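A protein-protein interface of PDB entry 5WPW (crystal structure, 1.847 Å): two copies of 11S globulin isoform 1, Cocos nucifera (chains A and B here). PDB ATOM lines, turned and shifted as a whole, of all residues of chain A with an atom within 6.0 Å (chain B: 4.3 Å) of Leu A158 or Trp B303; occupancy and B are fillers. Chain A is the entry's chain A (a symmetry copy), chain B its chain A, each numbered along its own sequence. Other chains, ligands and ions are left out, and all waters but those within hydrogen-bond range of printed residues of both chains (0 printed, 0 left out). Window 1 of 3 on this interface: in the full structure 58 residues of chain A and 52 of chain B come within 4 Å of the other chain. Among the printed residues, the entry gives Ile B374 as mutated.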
ATOM      1  N   PRO A  54     -17.561  -5.724  -8.202  1.00  0.00           N
ATOM      2  CA  PRO A  54     -18.540  -5.947  -7.130  1.00  0.00           C
ATOM      3  C   PRO A  54     -18.206  -5.161  -5.872  1.00  0.00           C
ATOM      4  O   PRO A  54     -17.047  -5.062  -5.459  1.00  0.00           O
ATOM      5  CB  PRO A  54     -18.475  -7.450  -6.890  1.00  0.00           C
ATOM      6  CG  PRO A  54     -17.130  -7.884  -7.469  1.00  0.00           C
ATOM      7  CD  PRO A  54     -16.920  -6.977  -8.640  1.00  0.00           C
ATOM      8  N   SER A  55     -19.249  -4.566  -5.284  1.00  0.00           N
ATOM      9  CA  SER A  55     -19.103  -3.762  -4.079  1.00  0.00           C
ATOM     10  C   SER A  55     -20.463  -3.671  -3.408  1.00  0.00           C
ATOM     11  O   SER A  55     -21.497  -3.961  -4.023  1.00  0.00           O
ATOM     12  CB  SER A  55     -18.543  -2.361  -4.380  1.00  0.00           C
ATOM     13  OG  SER A  55     -19.511  -1.493  -4.977  1.00  0.00           O
ATOM     14  N   MET A  56     -20.454  -3.282  -2.142  1.00  0.00           N
ATOM     15  CA  MET A  56     -21.698  -3.093  -1.412  1.00  0.00           C
ATOM     16  C   MET A  56     -21.598  -1.808  -0.610  1.00  0.00           C
ATOM     17  O   MET A  56     -20.504  -1.358  -0.257  1.00  0.00           O
ATOM     18  CB  MET A  56     -22.054  -4.299  -0.546  1.00  0.00           C
ATOM     19  CG  MET A  56     -21.046  -4.715   0.468  1.00  0.00           C
ATOM     20  SD  MET A  56     -21.373  -3.905   2.051  1.00  0.00           S
ATOM     21  CE  MET A  56     -20.218  -4.820   3.082  1.00  0.00           C
ATOM     22  N   GLY A 121     -25.944  -3.361   1.786  1.00  0.00           N
ATOM     23  CA  GLY A 121     -25.343  -4.602   2.212  1.00  0.00           C
ATOM     24  C   GLY A 121     -25.368  -5.741   1.217  1.00  0.00           C
ATOM     25  O   GLY A 121     -24.895  -6.832   1.560  1.00  0.00           O
ATOM     26  N   PHE A 122     -25.896  -5.537   0.002  1.00  0.00           N
ATOM     27  CA  PHE A 122     -25.917  -6.555  -1.046  1.00  0.00           C
ATOM     28  C   PHE A 122     -24.847  -6.255  -2.094  1.00  0.00           C
ATOM     29  O   PHE A 122     -24.787  -5.140  -2.611  1.00  0.00           O
ATOM     30  CB  PHE A 122     -27.278  -6.613  -1.767  1.00  0.00           C
ATOM     31  CG  PHE A 122     -28.415  -7.169  -0.934  1.00  0.00           C
ATOM     32  CD1 PHE A 122     -28.613  -6.769   0.371  1.00  0.00           C
ATOM     33  CD2 PHE A 122     -29.325  -8.063  -1.495  1.00  0.00           C
ATOM     34  CE1 PHE A 122     -29.671  -7.275   1.120  1.00  0.00           C
ATOM     35  CE2 PHE A 122     -30.382  -8.565  -0.757  1.00  0.00           C
ATOM     36  CZ  PHE A 122     -30.549  -8.175   0.563  1.00  0.00           C
ATOM     37  N   ALA A 123     -24.048  -7.262  -2.450  1.00  0.00           N
ATOM     38  CA  ALA A 123     -23.053  -7.101  -3.509  1.00  0.00           C
ATOM     39  C   ALA A 123     -23.697  -6.903  -4.880  1.00  0.00           C
ATOM     40  O   ALA A 123     -24.631  -7.618  -5.269  1.00  0.00           O
ATOM     41  CB  ALA A 123     -22.117  -8.310  -3.548  1.00  0.00           C
ATOM     42  N   PHE A 156     -17.887  -0.569   0.203  1.00  0.00           N
ATOM     43  CA  PHE A 156     -17.028  -1.693   0.553  1.00  0.00           C
ATOM     44  C   PHE A 156     -16.777  -2.483  -0.720  1.00  0.00           C
ATOM     45  O   PHE A 156     -17.668  -3.192  -1.191  1.00  0.00           O
ATOM     46  CB  PHE A 156     -17.675  -2.588   1.614  1.00  0.00           C
ATOM     47  CG  PHE A 156     -17.945  -1.900   2.942  1.00  0.00           C
ATOM     48  CD1 PHE A 156     -18.939  -0.949   3.061  1.00  0.00           C
ATOM     49  CD2 PHE A 156     -17.204  -2.233   4.075  1.00  0.00           C
ATOM     50  CE1 PHE A 156     -19.189  -0.334   4.306  1.00  0.00           C
ATOM     51  CE2 PHE A 156     -17.445  -1.639   5.300  1.00  0.00           C
ATOM     52  CZ  PHE A 156     -18.434  -0.685   5.420  1.00  0.00           C
ATOM     53  N   LEU A 157     -15.576  -2.366  -1.275  1.00  0.00           N
ATOM     54  CA  LEU A 157     -15.230  -3.088  -2.494  1.00  0.00           C
ATOM     55  C   LEU A 157     -14.954  -4.549  -2.175  1.00  0.00           C
ATOM     56  O   LEU A 157     -14.229  -4.854  -1.229  1.00  0.00           O
ATOM     57  CB  LEU A 157     -13.997  -2.473  -3.155  1.00  0.00           C
ATOM     58  CG  LEU A 157     -14.140  -1.050  -3.637  1.00  0.00           C
ATOM     59  CD1 LEU A 157     -12.757  -0.428  -3.717  1.00  0.00           C
ATOM     60  CD2 LEU A 157     -14.822  -1.060  -4.990  1.00  0.00           C
ATOM     61  N   LEU A 158     -15.551  -5.457  -2.951  1.00  0.00           N
ATOM     62  CA  LEU A 158     -15.184  -6.862  -2.834  1.00  0.00           C
ATOM     63  C   LEU A 158     -13.928  -7.177  -3.640  1.00  0.00           C
ATOM     64  O   LEU A 158     -13.231  -8.155  -3.348  1.00  0.00           O
ATOM     65  CB  LEU A 158     -16.341  -7.759  -3.300  1.00  0.00           C
ATOM     66  CG  LEU A 158     -17.591  -7.943  -2.430  1.00  0.00           C
ATOM     67  CD1 LEU A 158     -18.381  -9.177  -2.883  1.00  0.00           C
ATOM     68  CD2 LEU A 158     -17.242  -8.030  -0.971  1.00  0.00           C
ATOM     69  N   ALA A 159     -13.625  -6.371  -4.646  1.00  0.00           N
ATOM     70  CA  ALA A 159     -12.428  -6.556  -5.445  1.00  0.00           C
ATOM     71  C   ALA A 159     -11.936  -5.191  -5.882  1.00  0.00           C
ATOM     72  O   ALA A 159     -12.720  -4.247  -5.987  1.00  0.00           O
ATOM     73  CB  ALA A 159     -12.710  -7.441  -6.653  1.00  0.00           C
ATOM     74  N   GLY A 160     -10.633  -5.089  -6.134  1.00  0.00           N
ATOM     75  CA  GLY A 160     -10.078  -3.888  -6.731  1.00  0.00           C
ATOM     76  C   GLY A 160      -9.653  -2.825  -5.734  1.00  0.00           C
ATOM     77  O   GLY A 160      -9.450  -3.068  -4.544  1.00  0.00           O
ATOM     78  N   ASN A 178      -9.860  -3.020  -1.301  1.00  0.00           N
ATOM     79  CA  ASN A 178     -10.984  -3.920  -1.136  1.00  0.00           C
ATOM     80  C   ASN A 178     -10.905  -4.582   0.235  1.00  0.00           C
ATOM     81  O   ASN A 178      -9.863  -4.593   0.889  1.00  0.00           O
ATOM     82  CB  ASN A 178     -11.011  -4.954  -2.254  1.00  0.00           C
ATOM     83  CG  ASN A 178      -9.972  -6.023  -2.080  1.00  0.00           C
ATOM     84  OD1 ASN A 178     -10.231  -7.055  -1.467  1.00  0.00           O
ATOM     85  ND2 ASN A 178      -8.785  -5.788  -2.619  1.00  0.00           N
ATOM     86  N   ILE A 179     -12.041  -5.119   0.683  1.00  0.00           N
ATOM     87  CA  ILE A 179     -12.133  -5.571   2.070  1.00  0.00           C
ATOM     88  C   ILE A 179     -11.228  -6.763   2.326  1.00  0.00           C
ATOM     89  O   ILE A 179     -10.749  -6.950   3.453  1.00  0.00           O
ATOM     90  CB  ILE A 179     -13.589  -5.904   2.406  1.00  0.00           C
ATOM     91  CG1 ILE A 179     -14.138  -6.840   1.349  1.00  0.00           C
ATOM     92  CG2 ILE A 179     -14.395  -4.616   2.433  1.00  0.00           C
ATOM     93  CD1 ILE A 179     -15.246  -7.724   1.845  1.00  0.00           C
ATOM     94  N   LEU A 180     -10.988  -7.596   1.310  1.00  0.00           N
ATOM     95  CA  LEU A 180     -10.104  -8.744   1.505  1.00  0.00           C
ATOM     96  C   LEU A 180      -8.680  -8.309   1.827  1.00  0.00           C
ATOM     97  O   LEU A 180      -7.946  -9.043   2.502  1.00  0.00           O
ATOM     98  CB  LEU A 180     -10.118  -9.642   0.274  1.00  0.00           C
ATOM     99  CG  LEU A 180     -11.496 -10.129  -0.180  1.00  0.00           C
ATOM    100  CD1 LEU A 180     -11.340 -11.057  -1.380  1.00  0.00           C
ATOM    101  CD2 LEU A 180     -12.253 -10.810   0.969  1.00  0.00           C
ATOM    102  N   LEU A 202      -6.187 -12.238  -4.590  1.00  0.00           N
ATOM    103  CA  LEU A 202      -7.512 -11.733  -4.251  1.00  0.00           C
ATOM    104  C   LEU A 202      -7.434 -10.366  -3.591  1.00  0.00           C
ATOM    105  O   LEU A 202      -8.355  -9.558  -3.741  1.00  0.00           O
ATOM    106  CB  LEU A 202      -8.245 -12.719  -3.348  1.00  0.00           C
ATOM    107  CG  LEU A 202      -8.772 -13.930  -4.107  1.00  0.00           C
ATOM    108  CD1 LEU A 202      -9.245 -14.962  -3.123  1.00  0.00           C
ATOM    109  CD2 LEU A 202      -9.889 -13.553  -5.085  1.00  0.00           C
ATOM    110  N   HIS B 302     -17.402 -12.944   6.560  1.00  0.00           N
ATOM    111  CA  HIS B 302     -18.761 -12.473   6.339  1.00  0.00           C
ATOM    112  C   HIS B 302     -18.834 -11.014   6.743  1.00  0.00           C
ATOM    113  O   HIS B 302     -17.963 -10.499   7.462  1.00  0.00           O
ATOM    114  CB  HIS B 302     -19.799 -13.298   7.119  1.00  0.00           C
ATOM    115  CG  HIS B 302     -19.603 -13.270   8.612  1.00  0.00           C
ATOM    116  ND1 HIS B 302     -18.634 -14.021   9.250  1.00  0.00           N
ATOM    117  CD2 HIS B 302     -20.269 -12.606   9.591  1.00  0.00           C
ATOM    118  CE1 HIS B 302     -18.689 -13.791  10.549  1.00  0.00           C
ATOM    119  NE2 HIS B 302     -19.677 -12.945  10.785  1.00  0.00           N
ATOM    120  N   TRP B 303     -19.884 -10.343   6.270  1.00  0.00           N
ATOM    121  CA  TRP B 303     -20.258  -9.073   6.861  1.00  0.00           C
ATOM    122  C   TRP B 303     -21.710  -9.101   7.330  1.00  0.00           C
ATOM    123  O   TRP B 303     -22.543  -9.856   6.812  1.00  0.00           O
ATOM    124  CB  TRP B 303     -20.010  -7.919   5.875  1.00  0.00           C
ATOM    125  CG  TRP B 303     -20.915  -7.858   4.690  1.00  0.00           C
ATOM    126  CD1 TRP B 303     -22.136  -7.200   4.597  1.00  0.00           C
ATOM    127  CD2 TRP B 303     -20.660  -8.415   3.418  1.00  0.00           C
ATOM    128  NE1 TRP B 303     -22.641  -7.343   3.331  1.00  0.00           N
ATOM    129  CE2 TRP B 303     -21.753  -8.080   2.582  1.00  0.00           C
ATOM    130  CE3 TRP B 303     -19.607  -9.177   2.889  1.00  0.00           C
ATOM    131  CZ2 TRP B 303     -21.826  -8.489   1.243  1.00  0.00           C
ATOM    132  CZ3 TRP B 303     -19.673  -9.564   1.559  1.00  0.00           C
ATOM    133  CH2 TRP B 303     -20.780  -9.233   0.752  1.00  0.00           C
ATOM    134  N   ASN B 304     -21.998  -8.299   8.355  1.00  0.00           N
ATOM    135  CA  ASN B 304     -23.361  -8.132   8.820  1.00  0.00           C
ATOM    136  C   ASN B 304     -24.074  -7.154   7.907  1.00  0.00           C
ATOM    137  O   ASN B 304     -23.602  -6.033   7.701  1.00  0.00           O
ATOM    138  CB  ASN B 304     -23.392  -7.614  10.254  1.00  0.00           C
ATOM    139  CG  ASN B 304     -22.965  -8.665  11.238  1.00  0.00           C
ATOM    140  OD1 ASN B 304     -23.731  -9.572  11.555  1.00  0.00           O
ATOM    141  ND2 ASN B 304     -21.731  -8.566  11.711  1.00  0.00           N
ATOM    142  N   ILE B 305     -25.228  -7.573   7.405  1.00  0.00           N
ATOM    143  CA  ILE B 305     -25.923  -6.806   6.380  1.00  0.00           C
ATOM    144  C   ILE B 305     -26.683  -5.648   6.994  1.00  0.00           C
ATOM    145  O   ILE B 305     -26.579  -4.503   6.533  1.00  0.00           O
ATOM    146  CB  ILE B 305     -26.871  -7.716   5.582  1.00  0.00           C
ATOM    147  CG1 ILE B 305     -26.070  -8.627   4.647  1.00  0.00           C
ATOM    148  CG2 ILE B 305     -27.862  -6.887   4.796  1.00  0.00           C
ATOM    149  CD1 ILE B 305     -26.903  -9.718   4.059  1.00  0.00           C
ATOM    150  N   ASN B 346     -21.734  -4.036   8.135  1.00  0.00           N
ATOM    151  CA  ASN B 346     -21.067  -4.007   6.832  1.00  0.00           C
ATOM    152  C   ASN B 346     -19.579  -4.350   6.944  1.00  0.00           C
ATOM    153  O   ASN B 346     -18.980  -4.737   5.940  1.00  0.00           O
ATOM    154  CB  ASN B 346     -21.202  -2.643   6.134  1.00  0.00           C
ATOM    155  CG  ASN B 346     -22.497  -2.465   5.363  1.00  0.00           C
ATOM    156  OD1 ASN B 346     -23.355  -1.668   5.746  1.00  0.00           O
ATOM    157  ND2 ASN B 346     -22.606  -3.138   4.220  1.00  0.00           N
ATOM    158  N   PHE B 347     -18.955  -4.204   8.120  1.00  0.00           N
ATOM    159  CA  PHE B 347     -17.542  -4.585   8.247  1.00  0.00           C
ATOM    160  C   PHE B 347     -17.386  -6.082   8.030  1.00  0.00           C
ATOM    161  O   PHE B 347     -18.202  -6.873   8.489  1.00  0.00           O
ATOM    162  CB  PHE B 347     -16.978  -4.222   9.618  1.00  0.00           C
ATOM    163  CG  PHE B 347     -16.627  -2.768   9.767  1.00  0.00           C
ATOM    164  CD1 PHE B 347     -17.412  -1.784   9.166  1.00  0.00           C
ATOM    165  CD2 PHE B 347     -15.534  -2.374  10.527  1.00  0.00           C
ATOM    166  CE1 PHE B 347     -17.106  -0.438   9.298  1.00  0.00           C
ATOM    167  CE2 PHE B 347     -15.224  -1.014  10.683  1.00  0.00           C
ATOM    168  CZ  PHE B 347     -16.018  -0.044  10.069  1.00  0.00           C
ATOM    169  N   ALA B 348     -16.327  -6.479   7.333  1.00  0.00           N
ATOM    170  CA  ALA B 348     -16.106  -7.887   7.054  1.00  0.00           C
ATOM    171  C   ALA B 348     -15.302  -8.481   8.197  1.00  0.00           C
ATOM    172  O   ALA B 348     -14.379  -7.848   8.708  1.00  0.00           O
ATOM    173  CB  ALA B 348     -15.370  -8.082   5.723  1.00  0.00           C
ATOM    174  N   VAL B 371     -26.352 -12.113   7.883  1.00  0.00           N
ATOM    175  CA  VAL B 371     -24.989 -11.942   7.420  1.00  0.00           C
ATOM    176  C   VAL B 371     -24.909 -12.342   5.945  1.00  0.00           C
ATOM    177  O   VAL B 371     -25.747 -13.086   5.407  1.00  0.00           O
ATOM    178  CB  VAL B 371     -23.966 -12.763   8.240  1.00  0.00           C
ATOM    179  CG1 VAL B 371     -24.020 -12.386   9.732  1.00  0.00           C
ATOM    180  CG2 VAL B 371     -24.214 -14.239   8.018  1.00  0.00           C
ATOM    181  N   SER B 372     -23.858 -11.850   5.304  1.00  0.00           N
ATOM    182  CA  SER B 372     -23.467 -12.253   3.956  1.00  0.00           C
ATOM    183  C   SER B 372     -22.074 -12.876   4.012  1.00  0.00           C
ATOM    184  O   SER B 372     -21.103 -12.180   4.326  1.00  0.00           O
ATOM    185  CB  SER B 372     -23.451 -11.044   3.032  1.00  0.00           C
ATOM    186  OG  SER B 372     -23.118 -11.432   1.729  1.00  0.00           O
ATOM    187  N   ILE B 374     -18.608 -14.426   2.315  1.00  0.00           N
ATOM    188  CA  ILE B 374     -17.794 -14.116   1.140  1.00  0.00           C
ATOM    189  C   ILE B 374     -17.501 -15.366   0.328  1.00  0.00           C
ATOM    190  O   ILE B 374     -17.600 -15.336  -0.896  1.00  0.00           O
ATOM    191  CB  ILE B 374     -16.499 -13.399   1.576  1.00  0.00           C
ATOM    192  CG1 ILE B 374     -16.846 -12.104   2.304  1.00  0.00           C
ATOM    193  CG2 ILE B 374     -15.637 -13.042   0.385  1.00  0.00           C
ATOM    194  CD1 ILE B 374     -15.652 -11.278   2.737  1.00  0.00           C
ATOM    195  N   ALA B 380     -21.362 -14.470  -1.430  1.00  0.00           N
ATOM    196  CA  ALA B 380     -21.338 -13.473  -2.486  1.00  0.00           C
ATOM    197  C   ALA B 380     -20.545 -13.962  -3.692  1.00  0.00           C
ATOM    198  O   ALA B 380     -20.977 -13.797  -4.843  1.00  0.00           O
ATOM    199  CB  ALA B 380     -20.732 -12.183  -1.942  1.00  0.00           C
ATOM    200  N   MET B 384     -21.506 -15.111  -8.160  1.00  0.00           N
ATOM    201  CA  MET B 384     -21.008 -14.275  -9.240  1.00  0.00           C
ATOM    202  C   MET B 384     -20.476 -15.129 -10.385  1.00  0.00           C
ATOM    203  O   MET B 384     -19.901 -16.202 -10.158  1.00  0.00           O
ATOM    204  CB  MET B 384     -19.896 -13.355  -8.727  1.00  0.00           C
ATOM    205  CG  MET B 384     -20.452 -12.068  -8.091  1.00  0.00           C
ATOM    206  SD  MET B 384     -19.124 -11.119  -7.360  1.00  0.00           S
ATOM    207  CE  MET B 384     -20.095 -10.385  -5.999  1.00  0.00           C
ATOM    208  N   TYR B 393     -10.425  -9.852 -10.176  1.00  0.00           N
ATOM    209  CA  TYR B 393      -9.185 -10.127  -9.470  1.00  0.00           C
ATOM    210  C   TYR B 393      -8.008 -10.360 -10.414  1.00  0.00           C
ATOM    211  O   TYR B 393      -6.920 -10.685  -9.941  1.00  0.00           O
ATOM    212  CB  TYR B 393      -9.370 -11.350  -8.557  1.00  0.00           C
ATOM    213  CG  TYR B 393     -10.443 -11.172  -7.501  1.00  0.00           C
ATOM    214  CD1 TYR B 393     -10.247 -10.329  -6.424  1.00  0.00           C
ATOM    215  CD2 TYR B 393     -11.653 -11.850  -7.592  1.00  0.00           C
ATOM    216  CE1 TYR B 393     -11.231 -10.176  -5.447  1.00  0.00           C
ATOM    217  CE2 TYR B 393     -12.629 -11.701  -6.644  1.00  0.00           C
ATOM    218  CZ  TYR B 393     -12.425 -10.863  -5.579  1.00  0.00           C
ATOM    219  OH  TYR B 393     -13.432 -10.723  -4.641  1.00  0.00           O
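The indole nitrogen (NE1) of Trp B303 lies within hydrogen-bond range of the backbone carbonyl oxygen (O) of Gly A121, 2.9 Å away.
The side-chain amide nitrogen (ND2) of Asn B346 is in hydrogen-bond range of the side-chain sulfur (SD) of Met A56.
OH of Tyr B393 sits at hydrogen-bond distance from O of Leu A158 (2.9 Å).
Printed residues of chain A that touch a printed residue of chain B: Pro A54, Met A56, Gly A121, Ala A123, Phe A156, Leu A158, Ala A159, Ile A179, Leu A180 and Leu A202.
Among the printed residues, 19 pairs touch across the chains.
Among the printed residues, no Asp or Glu carboxylate lies within 4 Å of a Lys or Arg side-chain nitrogen of the other chain.
The backbone carbonyl oxygen (O) of Trp B303 is in hydrogen-bond range of the backbone NH (N) of Ser B372 (2.8 Å).
O of Asn B304 sits at hydrogen-bond distance from N of Asn B346 (2.8 Å).
O of Pro A54 is in hydrogen-bond range of N of Leu A158, 2.9 Å away.
The backbone carbonyl oxygen (O) of Met A56 sits at hydrogen-bond distance from the backbone NH (N) of Phe A156 (2.8 Å).
N of Ile A179 is in hydrogen-bond range of O of Leu A157 (2.9 Å).
OD1 of Asn A178 lies within hydrogen-bond range of N of Leu A180.
Of the printed residues of chain B, Leu A158 touches Trp B303, Ala B380, Met B384 and Tyr B393.
Of the printed residues of chain A, Trp B303 touches Met A56 (3.4 Å), Gly A121 (2.9 Å) and Leu A158 (3.8 Å).
Of the printed residues of chain A, Met B384 touches Pro A54 (3.5 Å), Ala A123 (3.8 Å) and Leu A158 (3.8 Å).
Printed residues of chain B within 4 Å of Met A56: Trp B303 and Asn B346.
Of the printed residues of chain A, Asn B346 touches Met A56, Gly A121 and Phe A156.
Printed residues of chain B within 4 Å of Ala A123: Met B384.
Of the printed residues of chain A, Tyr B393 touches Leu A158, Ala A159, Leu A180 and Leu A202.
The nearest printed residue of chain B that does not touch Leu A158 is Ile B374 (5.2 Å).
No position is printed for both chains.
Of the 19 pairs that touch across the chains among the printed residues, none has its exchanged pair printed and touching as well.
Met A56 touches Trp B303 (CE to CD1, 3.4 Å).
Gly A121 touches Ile B305 (O to CG1, 3.8 Å).
Asn B346 touches Gly A121.
CE2 of Phe A156 touches CD1 of Phe B347 (3.9 Å).
Leu A158 touches Trp B303.
Leu A158 touches Met B384 (CD1 to CE, 3.8 Å).
Ala A159 touches Tyr B393.
CD1 of Ile A179 touches CD1 of Ile B374 (3.7 Å).
CD1 of Leu A180 touches OH of Tyr B393 (3.9 Å).
Leu A202 touches Tyr B393 (O to CD1, 3.4 Å).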
